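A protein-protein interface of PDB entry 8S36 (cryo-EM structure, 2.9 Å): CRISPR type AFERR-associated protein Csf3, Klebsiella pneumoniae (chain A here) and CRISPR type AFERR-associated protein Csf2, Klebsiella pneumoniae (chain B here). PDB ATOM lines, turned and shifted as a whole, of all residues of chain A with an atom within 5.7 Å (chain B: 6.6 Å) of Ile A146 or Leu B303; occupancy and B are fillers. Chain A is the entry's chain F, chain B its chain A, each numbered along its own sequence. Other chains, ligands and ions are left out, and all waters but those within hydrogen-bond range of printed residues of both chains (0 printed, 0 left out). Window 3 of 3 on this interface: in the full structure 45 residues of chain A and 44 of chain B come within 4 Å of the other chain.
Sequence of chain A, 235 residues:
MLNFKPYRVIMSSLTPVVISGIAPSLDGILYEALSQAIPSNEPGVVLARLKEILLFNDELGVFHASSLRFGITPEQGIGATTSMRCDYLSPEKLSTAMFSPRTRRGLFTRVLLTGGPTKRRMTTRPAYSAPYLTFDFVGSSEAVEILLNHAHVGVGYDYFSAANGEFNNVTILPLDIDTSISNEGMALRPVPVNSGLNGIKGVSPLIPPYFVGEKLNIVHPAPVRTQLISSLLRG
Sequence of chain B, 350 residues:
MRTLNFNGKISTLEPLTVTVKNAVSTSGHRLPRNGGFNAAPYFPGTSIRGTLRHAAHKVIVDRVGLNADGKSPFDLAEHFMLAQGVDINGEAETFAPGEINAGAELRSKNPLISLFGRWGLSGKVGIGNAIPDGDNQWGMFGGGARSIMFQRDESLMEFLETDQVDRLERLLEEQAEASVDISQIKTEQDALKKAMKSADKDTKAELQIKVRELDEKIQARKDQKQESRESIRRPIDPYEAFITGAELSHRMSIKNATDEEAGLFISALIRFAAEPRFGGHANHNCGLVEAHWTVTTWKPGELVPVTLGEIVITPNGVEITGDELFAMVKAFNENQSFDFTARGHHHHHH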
ATOM      1  N   LEU A  34      10.237 -31.536 -26.961  1.00  0.00           N
ATOM      2  CA  LEU A  34      10.194 -30.802 -28.222  1.00  0.00           C
ATOM      3  C   LEU A  34       8.903 -31.050 -28.993  1.00  0.00           C
ATOM      4  O   LEU A  34       8.485 -30.195 -29.778  1.00  0.00           O
ATOM      5  CB  LEU A  34      11.398 -31.170 -29.082  1.00  0.00           C
ATOM      6  CG  LEU A  34      12.711 -30.516 -28.657  1.00  0.00           C
ATOM      7  CD1 LEU A  34      13.842 -31.125 -29.437  1.00  0.00           C
ATOM      8  CD2 LEU A  34      12.673 -29.008 -28.858  1.00  0.00           C
ATOM      9  N   ALA A  37       7.059 -28.263 -27.166  1.00  0.00           N
ATOM     10  CA  ALA A  37       7.569 -26.916 -27.409  1.00  0.00           C
ATOM     11  C   ALA A  37       7.193 -26.400 -28.792  1.00  0.00           C
ATOM     12  O   ALA A  37       6.513 -25.376 -28.924  1.00  0.00           O
ATOM     13  CB  ALA A  37       9.088 -26.902 -27.227  1.00  0.00           C
ATOM     14  N   ARG A  49      14.550 -31.032 -34.835  1.00  0.00           N
ATOM     15  CA  ARG A  49      14.828 -30.020 -33.823  1.00  0.00           C
ATOM     16  C   ARG A  49      15.568 -30.615 -32.632  1.00  0.00           C
ATOM     17  O   ARG A  49      16.342 -29.914 -31.972  1.00  0.00           O
ATOM     18  CB  ARG A  49      13.514 -29.368 -33.377  1.00  0.00           C
ATOM     19  CG  ARG A  49      13.608 -28.426 -32.174  1.00  0.00           C
ATOM     20  CD  ARG A  49      14.394 -27.162 -32.489  1.00  0.00           C
ATOM     21  NE  ARG A  49      13.562 -26.146 -33.124  1.00  0.00           N
ATOM     22  CZ  ARG A  49      12.623 -25.446 -32.502  1.00  0.00           C
ATOM     23  NH1 ARG A  49      12.364 -25.621 -31.215  1.00  0.00           N
ATOM     24  NH2 ARG A  49      11.925 -24.545 -33.188  1.00  0.00           N
ATOM     25  N   ILE A  53      19.632 -29.705 -30.533  1.00  0.00           N
ATOM     26  CA  ILE A  53      19.970 -29.570 -29.121  1.00  0.00           C
ATOM     27  C   ILE A  53      20.620 -30.817 -28.546  1.00  0.00           C
ATOM     28  O   ILE A  53      21.138 -30.760 -27.419  1.00  0.00           O
ATOM     29  CB  ILE A  53      18.731 -29.191 -28.278  1.00  0.00           C
ATOM     30  CG1 ILE A  53      17.613 -30.226 -28.441  1.00  0.00           C
ATOM     31  CG2 ILE A  53      18.224 -27.816 -28.678  1.00  0.00           C
ATOM     32  CD1 ILE A  53      16.619 -30.216 -27.301  1.00  0.00           C
ATOM     33  N   SER A 141      23.316 -27.527 -23.047  1.00  0.00           N
ATOM     34  CA  SER A 141      22.816 -27.582 -21.676  1.00  0.00           C
ATOM     35  C   SER A 141      21.627 -26.652 -21.466  1.00  0.00           C
ATOM     36  O   SER A 141      20.655 -27.031 -20.806  1.00  0.00           O
ATOM     37  CB  SER A 141      23.930 -27.231 -20.693  1.00  0.00           C
ATOM     38  OG  SER A 141      23.417 -26.516 -19.582  1.00  0.00           O
ATOM     39  N   GLU A 142      21.688 -25.428 -21.995  1.00  0.00           N
ATOM     40  CA  GLU A 142      20.603 -24.477 -21.762  1.00  0.00           C
ATOM     41  C   GLU A 142      19.280 -24.994 -22.321  1.00  0.00           C
ATOM     42  O   GLU A 142      18.243 -24.914 -21.651  1.00  0.00           O
ATOM     43  CB  GLU A 142      20.958 -23.097 -22.333  1.00  0.00           C
ATOM     44  CG  GLU A 142      20.942 -22.933 -23.854  1.00  0.00           C
ATOM     45  CD  GLU A 142      22.096 -23.635 -24.535  1.00  0.00           C
ATOM     46  OE1 GLU A 142      22.942 -24.218 -23.826  1.00  0.00           O
ATOM     47  OE2 GLU A 142      22.158 -23.604 -25.782  1.00  0.00           O
ATOM     48  N   ALA A 143      19.298 -25.538 -23.538  1.00  0.00           N
ATOM     49  CA  ALA A 143      18.064 -26.007 -24.161  1.00  0.00           C
ATOM     50  C   ALA A 143      17.468 -27.171 -23.382  1.00  0.00           C
ATOM     51  O   ALA A 143      16.260 -27.202 -23.110  1.00  0.00           O
ATOM     52  CB  ALA A 143      18.330 -26.409 -25.611  1.00  0.00           C
ATOM     53  N   VAL A 144      18.301 -28.146 -23.018  1.00  0.00           N
ATOM     54  CA  VAL A 144      17.799 -29.312 -22.302  1.00  0.00           C
ATOM     55  C   VAL A 144      17.310 -28.912 -20.917  1.00  0.00           C
ATOM     56  O   VAL A 144      16.312 -29.446 -20.421  1.00  0.00           O
ATOM     57  CB  VAL A 144      18.888 -30.396 -22.226  1.00  0.00           C
ATOM     58  CG1 VAL A 144      18.439 -31.537 -21.323  1.00  0.00           C
ATOM     59  CG2 VAL A 144      19.223 -30.897 -23.622  1.00  0.00           C
ATOM     60  N   GLU A 145      17.997 -27.969 -20.272  1.00  0.00           N
ATOM     61  CA  GLU A 145      17.538 -27.483 -18.977  1.00  0.00           C
ATOM     62  C   GLU A 145      16.177 -26.815 -19.103  1.00  0.00           C
ATOM     63  O   GLU A 145      15.270 -27.076 -18.303  1.00  0.00           O
ATOM     64  CB  GLU A 145      18.565 -26.509 -18.395  1.00  0.00           C
ATOM     65  CG  GLU A 145      18.147 -25.805 -17.105  1.00  0.00           C
ATOM     66  CD  GLU A 145      17.821 -26.769 -15.980  1.00  0.00           C
ATOM     67  OE1 GLU A 145      16.860 -27.554 -16.120  1.00  0.00           O
ATOM     68  OE2 GLU A 145      18.528 -26.740 -14.951  1.00  0.00           O
ATOM     69  N   ILE A 146      16.008 -25.970 -20.122  1.00  0.00           N
ATOM     70  CA  ILE A 146      14.733 -25.292 -20.327  1.00  0.00           C
ATOM     71  C   ILE A 146      13.629 -26.310 -20.559  1.00  0.00           C
ATOM     72  O   ILE A 146      12.537 -26.206 -19.988  1.00  0.00           O
ATOM     73  CB  ILE A 146      14.840 -24.296 -21.497  1.00  0.00           C
ATOM     74  CG1 ILE A 146      15.718 -23.106 -21.104  1.00  0.00           C
ATOM     75  CG2 ILE A 146      13.459 -23.813 -21.916  1.00  0.00           C
ATOM     76  CD1 ILE A 146      16.305 -22.366 -22.285  1.00  0.00           C
ATOM     77  N   LEU A 147      13.896 -27.315 -21.393  1.00  0.00           N
ATOM     78  CA  LEU A 147      12.885 -28.329 -21.670  1.00  0.00           C
ATOM     79  C   LEU A 147      12.521 -29.094 -20.403  1.00  0.00           C
ATOM     80  O   LEU A 147      11.343 -29.196 -20.042  1.00  0.00           O
ATOM     81  CB  LEU A 147      13.388 -29.289 -22.749  1.00  0.00           C
ATOM     82  CG  LEU A 147      13.444 -28.746 -24.178  1.00  0.00           C
ATOM     83  CD1 LEU A 147      14.098 -29.761 -25.100  1.00  0.00           C
ATOM     84  CD2 LEU A 147      12.057 -28.382 -24.680  1.00  0.00           C
ATOM     85  N   LEU A 148      13.524 -29.628 -19.706  1.00  0.00           N
ATOM     86  CA  LEU A 148      13.255 -30.458 -18.538  1.00  0.00           C
ATOM     87  C   LEU A 148      12.595 -29.668 -17.415  1.00  0.00           C
ATOM     88  O   LEU A 148      11.867 -30.249 -16.602  1.00  0.00           O
ATOM     89  CB  LEU A 148      14.551 -31.099 -18.044  1.00  0.00           C
ATOM     90  CG  LEU A 148      15.211 -32.085 -19.011  1.00  0.00           C
ATOM     91  CD1 LEU A 148      16.580 -32.493 -18.500  1.00  0.00           C
ATOM     92  CD2 LEU A 148      14.336 -33.309 -19.223  1.00  0.00           C
ATOM     93  N   ASN A 149      12.824 -28.355 -17.346  1.00  0.00           N
ATOM     94  CA  ASN A 149      12.271 -27.571 -16.248  1.00  0.00           C
ATOM     95  C   ASN A 149      10.898 -26.999 -16.568  1.00  0.00           C
ATOM     96  O   ASN A 149      10.027 -26.973 -15.691  1.00  0.00           O
ATOM     97  CB  ASN A 149      13.218 -26.423 -15.883  1.00  0.00           C
ATOM     98  CG  ASN A 149      14.197 -26.790 -14.780  1.00  0.00           C
ATOM     99  OD1 ASN A 149      14.045 -27.806 -14.103  1.00  0.00           O
ATOM    100  ND2 ASN A 149      15.206 -25.950 -14.590  1.00  0.00           N
ATOM    101  N   HIS A 150      10.677 -26.544 -17.798  1.00  0.00           N
ATOM    102  CA  HIS A 150       9.444 -25.867 -18.176  1.00  0.00           C
ATOM    103  C   HIS A 150       8.738 -26.603 -19.308  1.00  0.00           C
ATOM    104  O   HIS A 150       8.154 -25.992 -20.204  1.00  0.00           O
ATOM    105  CB  HIS A 150       9.730 -24.416 -18.564  1.00  0.00           C
ATOM    106  CG  HIS A 150       9.808 -23.482 -17.395  1.00  0.00           C
ATOM    107  ND1 HIS A 150       9.709 -23.910 -16.089  1.00  0.00           N
ATOM    108  CD2 HIS A 150       9.972 -22.139 -17.339  1.00  0.00           C
ATOM    109  CE1 HIS A 150       9.811 -22.871 -15.278  1.00  0.00           C
ATOM    110  NE2 HIS A 150       9.972 -21.785 -16.013  1.00  0.00           N
ATOM    111  N   ALA A 151       8.755 -27.933 -19.266  1.00  0.00           N
ATOM    112  CA  ALA A 151       7.897 -28.735 -20.124  1.00  0.00           C
ATOM    113  C   ALA A 151       7.311 -29.869 -19.299  1.00  0.00           C
ATOM    114  O   ALA A 151       7.849 -30.249 -18.257  1.00  0.00           O
ATOM    115  CB  ALA A 151       8.654 -29.296 -21.333  1.00  0.00           C
ATOM    116  N   TRP B 298       4.723 -21.904 -25.354  1.00  0.00           N
ATOM    117  CA  TRP B 298       6.034 -21.854 -25.984  1.00  0.00           C
ATOM    118  C   TRP B 298       6.005 -20.889 -27.161  1.00  0.00           C
ATOM    119  O   TRP B 298       5.103 -20.955 -28.002  1.00  0.00           O
ATOM    120  CB  TRP B 298       6.448 -23.245 -26.448  1.00  0.00           C
ATOM    121  CG  TRP B 298       6.830 -24.143 -25.327  1.00  0.00           C
ATOM    122  CD1 TRP B 298       6.022 -25.031 -24.680  1.00  0.00           C
ATOM    123  CD2 TRP B 298       8.125 -24.271 -24.734  1.00  0.00           C
ATOM    124  NE1 TRP B 298       6.733 -25.698 -23.716  1.00  0.00           N
ATOM    125  CE2 TRP B 298       8.026 -25.249 -23.727  1.00  0.00           C
ATOM    126  CE3 TRP B 298       9.358 -23.651 -24.952  1.00  0.00           C
ATOM    127  CZ2 TRP B 298       9.112 -25.620 -22.941  1.00  0.00           C
ATOM    128  CZ3 TRP B 298      10.433 -24.021 -24.167  1.00  0.00           C
ATOM    129  CH2 TRP B 298      10.302 -24.995 -23.175  1.00  0.00           C
ATOM    130  N   LYS B 299       6.983 -19.991 -27.208  1.00  0.00           N
ATOM    131  CA  LYS B 299       7.099 -19.085 -28.341  1.00  0.00           C
ATOM    132  C   LYS B 299       7.221 -19.899 -29.625  1.00  0.00           C
ATOM    133  O   LYS B 299       8.002 -20.860 -29.665  1.00  0.00           O
ATOM    134  CB  LYS B 299       8.320 -18.183 -28.179  1.00  0.00           C
ATOM    135  CG  LYS B 299       8.122 -17.033 -27.216  1.00  0.00           C
ATOM    136  CD  LYS B 299       9.256 -16.015 -27.305  1.00  0.00           C
ATOM    137  CE  LYS B 299       9.179 -15.150 -28.560  1.00  0.00           C
ATOM    138  NZ  LYS B 299       7.875 -14.444 -28.707  1.00  0.00           N
ATOM    139  N   GLY B 301       8.736 -21.439 -32.484  1.00  0.00           N
ATOM    140  CA  GLY B 301      10.039 -21.582 -33.096  1.00  0.00           C
ATOM    141  C   GLY B 301      11.223 -21.452 -32.161  1.00  0.00           C
ATOM    142  O   GLY B 301      12.361 -21.625 -32.614  1.00  0.00           O
ATOM    143  N   GLU B 302      11.004 -21.151 -30.880  1.00  0.00           N
ATOM    144  CA  GLU B 302      12.095 -21.053 -29.920  1.00  0.00           C
ATOM    145  C   GLU B 302      11.715 -21.770 -28.633  1.00  0.00           C
ATOM    146  O   GLU B 302      10.547 -22.080 -28.388  1.00  0.00           O
ATOM    147  CB  GLU B 302      12.460 -19.595 -29.609  1.00  0.00           C
ATOM    148  CG  GLU B 302      12.473 -18.678 -30.821  1.00  0.00           C
ATOM    149  CD  GLU B 302      11.102 -18.123 -31.144  1.00  0.00           C
ATOM    150  OE1 GLU B 302      10.106 -18.699 -30.662  1.00  0.00           O
ATOM    151  OE2 GLU B 302      11.020 -17.116 -31.878  1.00  0.00           O
ATOM    152  N   LEU B 303      12.730 -22.027 -27.811  1.00  0.00           N
ATOM    153  CA  LEU B 303      12.550 -22.650 -26.501  1.00  0.00           C
ATOM    154  C   LEU B 303      12.417 -21.587 -25.406  1.00  0.00           C
ATOM    155  O   LEU B 303      13.202 -21.536 -24.459  1.00  0.00           O
ATOM    156  CB  LEU B 303      13.705 -23.602 -26.209  1.00  0.00           C
ATOM    157  CG  LEU B 303      13.764 -24.928 -26.976  1.00  0.00           C
ATOM    158  CD1 LEU B 303      12.529 -25.769 -26.702  1.00  0.00           C
ATOM    159  CD2 LEU B 303      13.944 -24.715 -28.474  1.00  0.00           C
ATOM    160  N   VAL B 304      11.411 -20.729 -25.546  1.00  0.00           N
ATOM    161  CA  VAL B 304      11.169 -19.673 -24.562  1.00  0.00           C
ATOM    162  C   VAL B 304       9.706 -19.707 -24.128  1.00  0.00           C
ATOM    163  O   VAL B 304       8.821 -19.856 -24.983  1.00  0.00           O
ATOM    164  CB  VAL B 304      11.535 -18.295 -25.133  1.00  0.00           C
ATOM    165  CG1 VAL B 304      11.245 -17.202 -24.111  1.00  0.00           C
ATOM    166  CG2 VAL B 304      12.997 -18.266 -25.555  1.00  0.00           C
ATOM    167  N   PRO B 305       9.393 -19.574 -22.836  1.00  0.00           N
ATOM    168  CA  PRO B 305       7.988 -19.403 -22.444  1.00  0.00           C
ATOM    169  C   PRO B 305       7.523 -17.958 -22.555  1.00  0.00           C
ATOM    170  O   PRO B 305       8.228 -17.022 -22.167  1.00  0.00           O
ATOM    171  CB  PRO B 305       7.960 -19.873 -20.981  1.00  0.00           C
ATOM    172  CG  PRO B 305       9.272 -20.525 -20.731  1.00  0.00           C
ATOM    173  CD  PRO B 305      10.234 -19.897 -21.672  1.00  0.00           C
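The guanidinium group (NH2) of Arg A49 sits at hydrogen-bond distance from the backbone carbonyl oxygen (O) of Gly B301 (3.0 Å).
Ile A146 touches two residues of chain B.
Of chain A, only Leu A34 (3.9 Å), Ala A37 (3.7 Å), Arg A49 (3.3 Å), Ile A146 (3.4 Å) and Leu A147 (3.3 Å) come within 4 Å of Leu B303.
Of the printed residues of chain A, Gly B301 touches Arg A49 (3.0 Å).
Of the printed residues of chain A, Trp B298 touches Ala A37 (3.3 Å), Ile A146 (3.6 Å) and His A150 (2.9 Å).
Val B304 touches none of the printed residues of chain A.
Glu B302 touches none of the printed residues of chain A.
The nearest residue of chain B that does not touch Ile A146 is Pro B305 (5.1 Å).
The nearest residue of chain A that does not touch Leu B303 is Ala A143 (5.0 Å).
Of the 15 printed residues of chain A, 6 touch a printed residue of chain B.
Printed residues of chain A that touch a printed residue of chain B: Leu A34, Ala A37, Arg A49, Ile A146, Leu A147 and His A150.
Hydrophobic or aromatic side chains of chain A within 4 Å of the printed part of chain B: Leu A34, Ala A37, Ile A146, Leu A147 and His A150.
Of the 7 printed residues of chain B, 4 touch a printed residue of chain A.
Hydrophobic or aromatic side chains of chain B within 4 Å of the printed part of chain A: Trp B298, Leu B303 and Pro B305.
Among the printed residues, 10 pairs touch across the chains.
Among the printed residues, no Asp or Glu carboxylate lies within 4 Å of a Lys or Arg side-chain nitrogen of the other chain.
CD1 of Leu B303 touches CD2 of Leu A34 (3.9 Å).
Ala A37 touches Trp B298 (O to CB, 3.3 Å).
Ala A37 touches Leu B303 (CB to CD1, 3.7 Å).
Arg A49 touches Leu B303 (NH1 to CD2, 3.3 Å).
Ile A146 touches Trp B298 (CG2 to CH2, 3.6 Å).
Ile A146 touches Leu B303.
CD2 of Leu A147 touches CD1 of Leu B303, at 3.3 Å.
His A150 touches Trp B298.
His A150 touches Pro B305 (CD2 to CG, 3.8 Å).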
